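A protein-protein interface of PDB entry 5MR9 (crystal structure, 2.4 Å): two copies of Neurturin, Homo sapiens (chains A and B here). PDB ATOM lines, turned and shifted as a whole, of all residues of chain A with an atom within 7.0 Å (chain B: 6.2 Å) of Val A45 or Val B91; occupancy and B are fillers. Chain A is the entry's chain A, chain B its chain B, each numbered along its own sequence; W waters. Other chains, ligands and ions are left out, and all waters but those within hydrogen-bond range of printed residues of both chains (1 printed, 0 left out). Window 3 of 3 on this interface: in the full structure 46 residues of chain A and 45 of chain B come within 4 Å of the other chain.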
ATOM      1  N   ALA A  42     -21.434  15.288 -12.045  1.00  0.00           N
ATOM      2  CA  ALA A  42     -20.957  16.372 -12.928  1.00  0.00           C
ATOM      3  C   ALA A  42     -19.688  15.958 -13.670  1.00  0.00           C
ATOM      4  O   ALA A  42     -18.739  15.466 -13.059  1.00  0.00           O
ATOM      5  CB  ALA A  42     -20.749  17.679 -12.166  1.00  0.00           C
ATOM      6  N   ALA A  43     -19.688  16.126 -14.994  1.00  0.00           N
ATOM      7  CA  ALA A  43     -18.566  15.749 -15.849  1.00  0.00           C
ATOM      8  C   ALA A  43     -17.217  16.278 -15.347  1.00  0.00           C
ATOM      9  O   ALA A  43     -17.097  17.462 -15.029  1.00  0.00           O
ATOM     10  CB  ALA A  43     -18.818  16.224 -17.262  1.00  0.00           C
ATOM     11  N   ARG A  44     -16.222  15.381 -15.236  1.00  0.00           N
ATOM     12  CA  ARG A  44     -14.873  15.738 -14.815  1.00  0.00           C
ATOM     13  C   ARG A  44     -14.207  16.514 -15.955  1.00  0.00           C
ATOM     14  O   ARG A  44     -14.539  16.285 -17.124  1.00  0.00           O
ATOM     15  CB  ARG A  44     -14.030  14.496 -14.500  1.00  0.00           C
ATOM     16  CG  ARG A  44     -14.373  13.784 -13.190  1.00  0.00           C
ATOM     17  CD  ARG A  44     -13.340  12.725 -12.818  1.00  0.00           C
ATOM     18  NE  ARG A  44     -12.051  13.322 -12.456  1.00  0.00           N
ATOM     19  CZ  ARG A  44     -11.451  13.183 -11.279  1.00  0.00           C
ATOM     20  NH1 ARG A  44     -10.286  13.767 -11.051  1.00  0.00           N
ATOM     21  NH2 ARG A  44     -12.001  12.436 -10.330  1.00  0.00           N
ATOM     22  N   VAL A  45     -13.265  17.426 -15.603  1.00  0.00           N
ATOM     23  CA  VAL A  45     -12.508  18.303 -16.519  1.00  0.00           C
ATOM     24  C   VAL A  45     -11.689  17.460 -17.547  1.00  0.00           C
ATOM     25  O   VAL A  45     -11.719  17.737 -18.753  1.00  0.00           O
ATOM     26  CB  VAL A  45     -11.741  19.441 -15.759  1.00  0.00           C
ATOM     27  CG1 VAL A  45     -10.270  19.128 -15.526  1.00  0.00           C
ATOM     28  CG2 VAL A  45     -11.961  20.797 -16.421  1.00  0.00           C
ATOM     29  N   TYR A  46     -11.172  16.304 -17.055  1.00  0.00           N
ATOM     30  CA  TYR A  46     -10.460  15.266 -17.788  1.00  0.00           C
ATOM     31  C   TYR A  46     -11.376  14.617 -18.854  1.00  0.00           C
ATOM     32  O   TYR A  46     -10.984  14.535 -20.020  1.00  0.00           O
ATOM     33  CB  TYR A  46      -9.916  14.208 -16.797  1.00  0.00           C
ATOM     34  CG  TYR A  46      -9.465  12.908 -17.461  1.00  0.00           C
ATOM     35  CD1 TYR A  46      -8.185  12.772 -17.988  1.00  0.00           C
ATOM     36  CD2 TYR A  46     -10.336  11.814 -17.558  1.00  0.00           C
ATOM     37  CE1 TYR A  46      -7.779  11.596 -18.609  1.00  0.00           C
ATOM     38  CE2 TYR A  46      -9.944  10.644 -18.208  1.00  0.00           C
ATOM     39  CZ  TYR A  46      -8.668  10.540 -18.719  1.00  0.00           C
ATOM     40  OH  TYR A  46      -8.287   9.379 -19.332  1.00  0.00           O
ATOM     41  N   ASP A  47     -12.612  14.226 -18.441  1.00  0.00           N
ATOM     42  CA  ASP A  47     -13.626  13.600 -19.302  1.00  0.00           C
ATOM     43  C   ASP A  47     -14.093  14.515 -20.440  1.00  0.00           C
ATOM     44  O   ASP A  47     -14.215  14.059 -21.580  1.00  0.00           O
ATOM     45  CB  ASP A  47     -14.820  13.019 -18.491  1.00  0.00           C
ATOM     46  CG  ASP A  47     -14.528  11.725 -17.753  1.00  0.00           C
ATOM     47  OD1 ASP A  47     -13.620  10.997 -18.181  1.00  0.00           O
ATOM     48  OD2 ASP A  47     -15.240  11.430 -16.760  1.00  0.00           O
ATOM     49  N   LEU A  48     -14.315  15.807 -20.125  1.00  0.00           N
ATOM     50  CA  LEU A  48     -14.759  16.869 -21.043  1.00  0.00           C
ATOM     51  C   LEU A  48     -13.721  17.120 -22.149  1.00  0.00           C
ATOM     52  O   LEU A  48     -14.053  17.126 -23.337  1.00  0.00           O
ATOM     53  CB  LEU A  48     -15.077  18.168 -20.252  1.00  0.00           C
ATOM     54  CG  LEU A  48     -16.528  18.602 -20.157  1.00  0.00           C
ATOM     55  CD1 LEU A  48     -17.503  17.417 -20.266  1.00  0.00           C
ATOM     56  CD2 LEU A  48     -16.775  19.360 -18.850  1.00  0.00           C
ATOM     57  N   GLY A  49     -12.471  17.309 -21.719  1.00  0.00           N
ATOM     58  CA  GLY A  49     -11.303  17.502 -22.572  1.00  0.00           C
ATOM     59  C   GLY A  49     -11.088  16.328 -23.515  1.00  0.00           C
ATOM     60  O   GLY A  49     -10.850  16.512 -24.711  1.00  0.00           O
ATOM     61  N   LEU A  50     -11.239  15.100 -22.975  1.00  0.00           N
ATOM     62  CA  LEU A  50     -11.131  13.813 -23.689  1.00  0.00           C
ATOM     63  C   LEU A  50     -12.199  13.609 -24.778  1.00  0.00           C
ATOM     64  O   LEU A  50     -11.844  13.179 -25.875  1.00  0.00           O
ATOM     65  CB  LEU A  50     -11.098  12.624 -22.704  1.00  0.00           C
ATOM     66  CG  LEU A  50     -10.464  11.312 -23.141  1.00  0.00           C
ATOM     67  CD1 LEU A  50      -9.061  11.508 -23.716  1.00  0.00           C
ATOM     68  CD2 LEU A  50     -10.322  10.407 -21.952  1.00  0.00           C
ATOM     69  N   LEU B  22     -12.943  23.865 -22.875  1.00  0.00           N
ATOM     70  CA  LEU B  22     -13.229  24.155 -21.468  1.00  0.00           C
ATOM     71  C   LEU B  22     -13.607  25.629 -21.268  1.00  0.00           C
ATOM     72  O   LEU B  22     -14.029  26.022 -20.179  1.00  0.00           O
ATOM     73  CB  LEU B  22     -12.054  23.724 -20.561  1.00  0.00           C
ATOM     74  CG  LEU B  22     -11.699  22.226 -20.573  1.00  0.00           C
ATOM     75  CD1 LEU B  22     -10.389  21.968 -19.885  1.00  0.00           C
ATOM     76  CD2 LEU B  22     -12.797  21.380 -19.954  1.00  0.00           C
ATOM     77  N   TYR B  24     -11.504  28.293 -22.001  1.00  0.00           N
ATOM     78  CA  TYR B  24     -10.339  29.127 -21.736  1.00  0.00           C
ATOM     79  C   TYR B  24      -9.828  29.732 -23.035  1.00  0.00           C
ATOM     80  O   TYR B  24      -9.675  29.020 -24.032  1.00  0.00           O
ATOM     81  CB  TYR B  24      -9.224  28.325 -21.046  1.00  0.00           C
ATOM     82  CG  TYR B  24      -9.565  27.812 -19.667  1.00  0.00           C
ATOM     83  CD1 TYR B  24      -9.488  28.648 -18.555  1.00  0.00           C
ATOM     84  CD2 TYR B  24      -9.879  26.475 -19.456  1.00  0.00           C
ATOM     85  CE1 TYR B  24      -9.760  28.172 -17.273  1.00  0.00           C
ATOM     86  CE2 TYR B  24     -10.162  25.989 -18.181  1.00  0.00           C
ATOM     87  CZ  TYR B  24     -10.094  26.841 -17.091  1.00  0.00           C
ATOM     88  OH  TYR B  24     -10.359  26.364 -15.829  1.00  0.00           O
ATOM     89  N   PHE B  32      -1.298  16.491 -22.603  1.00  0.00           N
ATOM     90  CA  PHE B  32      -2.495  15.846 -22.080  1.00  0.00           C
ATOM     91  C   PHE B  32      -2.245  14.351 -21.953  1.00  0.00           C
ATOM     92  O   PHE B  32      -1.869  13.695 -22.928  1.00  0.00           O
ATOM     93  CB  PHE B  32      -3.727  16.159 -22.947  1.00  0.00           C
ATOM     94  CG  PHE B  32      -5.024  15.620 -22.387  1.00  0.00           C
ATOM     95  CD1 PHE B  32      -5.659  16.252 -21.324  1.00  0.00           C
ATOM     96  CD2 PHE B  32      -5.620  14.493 -22.936  1.00  0.00           C
ATOM     97  CE1 PHE B  32      -6.860  15.754 -20.812  1.00  0.00           C
ATOM     98  CE2 PHE B  32      -6.816  13.994 -22.421  1.00  0.00           C
ATOM     99  CZ  PHE B  32      -7.425  14.622 -21.356  1.00  0.00           C
ATOM    100  N   GLU B  76      -3.170  13.993 -12.246  1.00  0.00           N
ATOM    101  CA  GLU B  76      -2.159  15.036 -12.124  1.00  0.00           C
ATOM    102  C   GLU B  76      -2.845  16.196 -11.389  1.00  0.00           C
ATOM    103  O   GLU B  76      -3.955  16.587 -11.750  1.00  0.00           O
ATOM    104  CB  GLU B  76      -1.629  15.432 -13.521  1.00  0.00           C
ATOM    105  CG  GLU B  76      -1.308  16.906 -13.705  1.00  0.00           C
ATOM    106  CD  GLU B  76      -2.167  17.583 -14.754  1.00  0.00           C
ATOM    107  OE1 GLU B  76      -1.628  17.883 -15.846  1.00  0.00           O
ATOM    108  OE2 GLU B  76      -3.377  17.794 -14.502  1.00  0.00           O
ATOM    109  N   ASP B  77      -2.229  16.653 -10.297  1.00  0.00           N
ATOM    110  CA  ASP B  77      -2.765  17.689  -9.420  1.00  0.00           C
ATOM    111  C   ASP B  77      -3.309  18.920 -10.133  1.00  0.00           C
ATOM    112  O   ASP B  77      -4.482  19.244  -9.938  1.00  0.00           O
ATOM    113  CB  ASP B  77      -1.748  18.057  -8.336  1.00  0.00           C
ATOM    114  CG  ASP B  77      -0.391  18.533  -8.826  1.00  0.00           C
ATOM    115  OD1 ASP B  77      -0.049  18.272 -10.013  1.00  0.00           O
ATOM    116  OD2 ASP B  77       0.336  19.153  -8.027  1.00  0.00           O
ATOM    117  N   GLU B  78      -2.484  19.571 -10.993  1.00  0.00           N
ATOM    118  CA  GLU B  78      -2.878  20.767 -11.750  1.00  0.00           C
ATOM    119  C   GLU B  78      -2.051  21.117 -12.986  1.00  0.00           C
ATOM    120  O   GLU B  78      -0.923  20.651 -13.148  1.00  0.00           O
ATOM    121  CB  GLU B  78      -3.028  22.008 -10.844  1.00  0.00           C
ATOM    122  CG  GLU B  78      -1.785  22.413 -10.064  1.00  0.00           C
ATOM    123  CD  GLU B  78      -1.884  23.758  -9.366  1.00  0.00           C
ATOM    124  OE1 GLU B  78      -2.286  24.744 -10.025  1.00  0.00           O
ATOM    125  OE2 GLU B  78      -1.508  23.839  -8.174  1.00  0.00           O
ATOM    126  N   VAL B  79      -2.645  21.957 -13.860  1.00  0.00           N
ATOM    127  CA  VAL B  79      -2.048  22.534 -15.072  1.00  0.00           C
ATOM    128  C   VAL B  79      -2.271  24.026 -14.984  1.00  0.00           C
ATOM    129  O   VAL B  79      -3.395  24.479 -14.747  1.00  0.00           O
ATOM    130  CB  VAL B  79      -2.579  22.028 -16.445  1.00  0.00           C
ATOM    131  CG1 VAL B  79      -1.472  22.059 -17.493  1.00  0.00           C
ATOM    132  CG2 VAL B  79      -3.189  20.644 -16.358  1.00  0.00           C
ATOM    133  N   SER B  80      -1.209  24.785 -15.205  1.00  0.00           N
ATOM    134  CA  SER B  80      -1.256  26.233 -15.151  1.00  0.00           C
ATOM    135  C   SER B  80      -0.847  26.835 -16.477  1.00  0.00           C
ATOM    136  O   SER B  80       0.054  26.320 -17.146  1.00  0.00           O
ATOM    137  CB  SER B  80      -0.374  26.746 -14.020  1.00  0.00           C
ATOM    138  OG  SER B  80      -0.949  26.431 -12.762  1.00  0.00           O
ATOM    139  N   PHE B  81      -1.532  27.914 -16.871  1.00  0.00           N
ATOM    140  CA  PHE B  81      -1.296  28.606 -18.133  1.00  0.00           C
ATOM    141  C   PHE B  81      -1.754  30.068 -18.084  1.00  0.00           C
ATOM    142  O   PHE B  81      -2.481  30.472 -17.177  1.00  0.00           O
ATOM    143  CB  PHE B  81      -1.976  27.856 -19.307  1.00  0.00           C
ATOM    144  CG  PHE B  81      -3.456  27.634 -19.150  1.00  0.00           C
ATOM    145  CD1 PHE B  81      -4.370  28.603 -19.557  1.00  0.00           C
ATOM    146  CD2 PHE B  81      -3.941  26.462 -18.587  1.00  0.00           C
ATOM    147  CE1 PHE B  81      -5.741  28.404 -19.391  1.00  0.00           C
ATOM    148  CE2 PHE B  81      -5.312  26.262 -18.433  1.00  0.00           C
ATOM    149  CZ  PHE B  81      -6.202  27.231 -18.835  1.00  0.00           C
ATOM    150  N   HIS B  89      -4.378  31.002 -15.079  1.00  0.00           N
ATOM    151  CA  HIS B  89      -5.433  30.034 -14.810  1.00  0.00           C
ATOM    152  C   HIS B  89      -4.856  28.735 -14.347  1.00  0.00           C
ATOM    153  O   HIS B  89      -3.778  28.335 -14.790  1.00  0.00           O
ATOM    154  CB  HIS B  89      -6.266  29.776 -16.070  1.00  0.00           C
ATOM    155  CG  HIS B  89      -7.141  30.918 -16.451  1.00  0.00           C
ATOM    156  ND1 HIS B  89      -8.336  31.140 -15.813  1.00  0.00           N
ATOM    157  CD2 HIS B  89      -6.970  31.857 -17.406  1.00  0.00           C
ATOM    158  CE1 HIS B  89      -8.856  32.211 -16.389  1.00  0.00           C
ATOM    159  NE2 HIS B  89      -8.069  32.678 -17.352  1.00  0.00           N
ATOM    160  N   THR B  90      -5.589  28.067 -13.462  1.00  0.00           N
ATOM    161  CA  THR B  90      -5.229  26.758 -12.949  1.00  0.00           C
ATOM    162  C   THR B  90      -6.361  25.792 -13.223  1.00  0.00           C
ATOM    163  O   THR B  90      -7.526  26.106 -12.957  1.00  0.00           O
ATOM    164  CB  THR B  90      -4.762  26.808 -11.481  1.00  0.00           C
ATOM    165  OG1 THR B  90      -4.345  25.496 -11.101  1.00  0.00           O
ATOM    166  CG2 THR B  90      -5.845  27.316 -10.515  1.00  0.00           C
ATOM    167  N   VAL B  91      -6.017  24.644 -13.818  1.00  0.00           N
ATOM    168  CA  VAL B  91      -6.952  23.567 -14.135  1.00  0.00           C
ATOM    169  C   VAL B  91      -6.532  22.381 -13.292  1.00  0.00           C
ATOM    170  O   VAL B  91      -5.398  21.916 -13.401  1.00  0.00           O
ATOM    171  CB  VAL B  91      -7.025  23.213 -15.649  1.00  0.00           C
ATOM    172  CG1 VAL B  91      -8.115  22.181 -15.914  1.00  0.00           C
ATOM    173  CG2 VAL B  91      -7.283  24.451 -16.487  1.00  0.00           C
ATOM    174  N   HIS B  92      -7.439  21.922 -12.427  1.00  0.00           N
ATOM    175  CA  HIS B  92      -7.180  20.803 -11.528  1.00  0.00           C
ATOM    176  C   HIS B  92      -7.696  19.495 -12.078  1.00  0.00           C
ATOM    177  O   HIS B  92      -8.821  19.434 -12.575  1.00  0.00           O
ATOM    178  CB  HIS B  92      -7.765  21.068 -10.133  1.00  0.00           C
ATOM    179  CG  HIS B  92      -7.000  22.095  -9.355  1.00  0.00           C
ATOM    180  ND1 HIS B  92      -7.536  23.338  -9.082  1.00  0.00           N
ATOM    181  CD2 HIS B  92      -5.767  22.019  -8.800  1.00  0.00           C
ATOM    182  CE1 HIS B  92      -6.609  23.983  -8.391  1.00  0.00           C
ATOM    183  NE2 HIS B  92      -5.522  23.234  -8.211  1.00  0.00           N
ATOM    184  N   GLU B  93      -6.868  18.441 -11.950  1.00  0.00           N
ATOM    185  CA  GLU B  93      -7.150  17.062 -12.356  1.00  0.00           C
ATOM    186  C   GLU B  93      -7.445  16.904 -13.865  1.00  0.00           C
ATOM    187  O   GLU B  93      -8.293  16.102 -14.255  1.00  0.00           O
ATOM    188  CB  GLU B  93      -8.217  16.406 -11.444  1.00  0.00           C
ATOM    189  CG  GLU B  93      -7.954  16.610  -9.956  1.00  0.00           C
ATOM    190  CD  GLU B  93      -8.275  15.443  -9.043  1.00  0.00           C
ATOM    191  OE1 GLU B  93      -9.477  15.161  -8.833  1.00  0.00           O
ATOM    192  OE2 GLU B  93      -7.324  14.856  -8.481  1.00  0.00           O
ATOM    193  N   LEU B  94      -6.705  17.649 -14.706  1.00  0.00           N
ATOM    194  CA  LEU B  94      -6.859  17.617 -16.156  1.00  0.00           C
ATOM    195  C   LEU B  94      -6.272  16.350 -16.778  1.00  0.00           C
ATOM    196  O   LEU B  94      -6.886  15.786 -17.677  1.00  0.00           O
ATOM    197  CB  LEU B  94      -6.309  18.905 -16.810  1.00  0.00           C
ATOM    198  CG  LEU B  94      -6.498  19.085 -18.336  1.00  0.00           C
ATOM    199  CD1 LEU B  94      -7.961  19.293 -18.705  1.00  0.00           C
ATOM    200  CD2 LEU B  94      -5.693  20.252 -18.850  1.00  0.00           C
ATOM    201  N   SER B  95      -5.112  15.890 -16.285  1.00  0.00           N
ATOM    202  CA  SER B  95      -4.453  14.699 -16.810  1.00  0.00           C
ATOM    203  C   SER B  95      -4.463  13.523 -15.843  1.00  0.00           C
ATOM    204  O   SER B  95      -4.466  13.705 -14.625  1.00  0.00           O
ATOM    205  CB  SER B  95      -3.017  15.015 -17.221  1.00  0.00           C
ATOM    206  OG  SER B  95      -2.963  16.010 -18.227  1.00  0.00           O
HETATM  207  O   HOH W   1     -10.863  15.578 -13.667  1.00  0.00           O
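Among the printed residues, merely in contact across the chains: Val A45 with Leu B22 (3.7 Å), Val A45 with Val B91 (3.8 Å), Val A45 with His B92 (3.3 Å), Val A45 with Glu B93 (3.8 Å), Val A45 with Leu B94 (3.8 Å), Tyr A46 with Phe B32 (3.8 Å), Tyr A46 with Glu B93 (3.6 Å), Tyr A46 with Leu B94 (3.3 Å), Leu A48 with Leu B22 (3.95 Å) and Leu A50 with Phe B32 (3.6 Å).
Val A45 touches just these residues of chain B: Leu B22, Val B91, His B92, Glu B93 and Leu B94.
Of chain A, only Val A45 (3.8 Å) comes within 4 Å of Val B91.
Printed residues of chain A within 4 Å of Phe B32: Tyr A46 (3.8 Å) and Leu A50 (3.6 Å).
Of the printed residues of chain A, His B92 touches Val A45 (3.3 Å).
Of the printed residues of chain B, Tyr A46 touches Phe B32, Glu B93 and Leu B94.
Of the printed residues of chain A, Glu B93 touches Arg A44 (2.7 Å), Val A45 (3.8 Å) and Tyr A46 (3.6 Å).
Printed residues of chain B within 4 Å of Leu A50: Phe B32.
Val B79 touches none of the printed residues of chain A.
Ala A42 touches none of the printed residues of chain B.
The nearest residue of chain B that does not touch Val A45 is Phe B32 (5.6 Å).
The nearest printed residue of chain A that does not touch Leu B94 is Gly A49 (5.4 Å).
Water W1 lies within hydrogen-bond range of O of Glu B93 (2.7 Å), NE of Arg A44 (2.8 Å) and N of Tyr A46 (3.5 Å).
The guanidinium group (NH1) of Arg A44 lies within salt-bridge range of the side-chain carboxylate (OE1) of Glu B93 (2.7 Å).
The backbone carbonyl oxygen (O) of Glu B76 sits close to the backbone NH (N) of Glu B93 (3.5 Å).
N of Glu B93 is in hydrogen-bond range of O of Asp B77 (3.2 Å).
The side-chain carboxylate (OE2) of Glu B76 lies within hydrogen-bond range of the backbone NH (N) of Leu B94, 3.3 Å away.
N of Val B91 sits at hydrogen-bond distance from O of Val B79 (2.8 Å).
No position is printed for both chains.
Of the 9 printed residues of chain A, 5 touch a printed residue of chain B.
Hydrophobic or aromatic side chains of chain A within 4 Å of the printed part of chain B: Val A45, Tyr A46, Leu A48 and Leu A50.
Of the 16 printed residues of chain B, 6 touch a printed residue of chain A.
Among the printed residues, Asp or Glu carboxylates within 4 Å of a Lys or Arg side-chain nitrogen of the other chain: Arg A44 with Glu B93 (2.7 Å).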
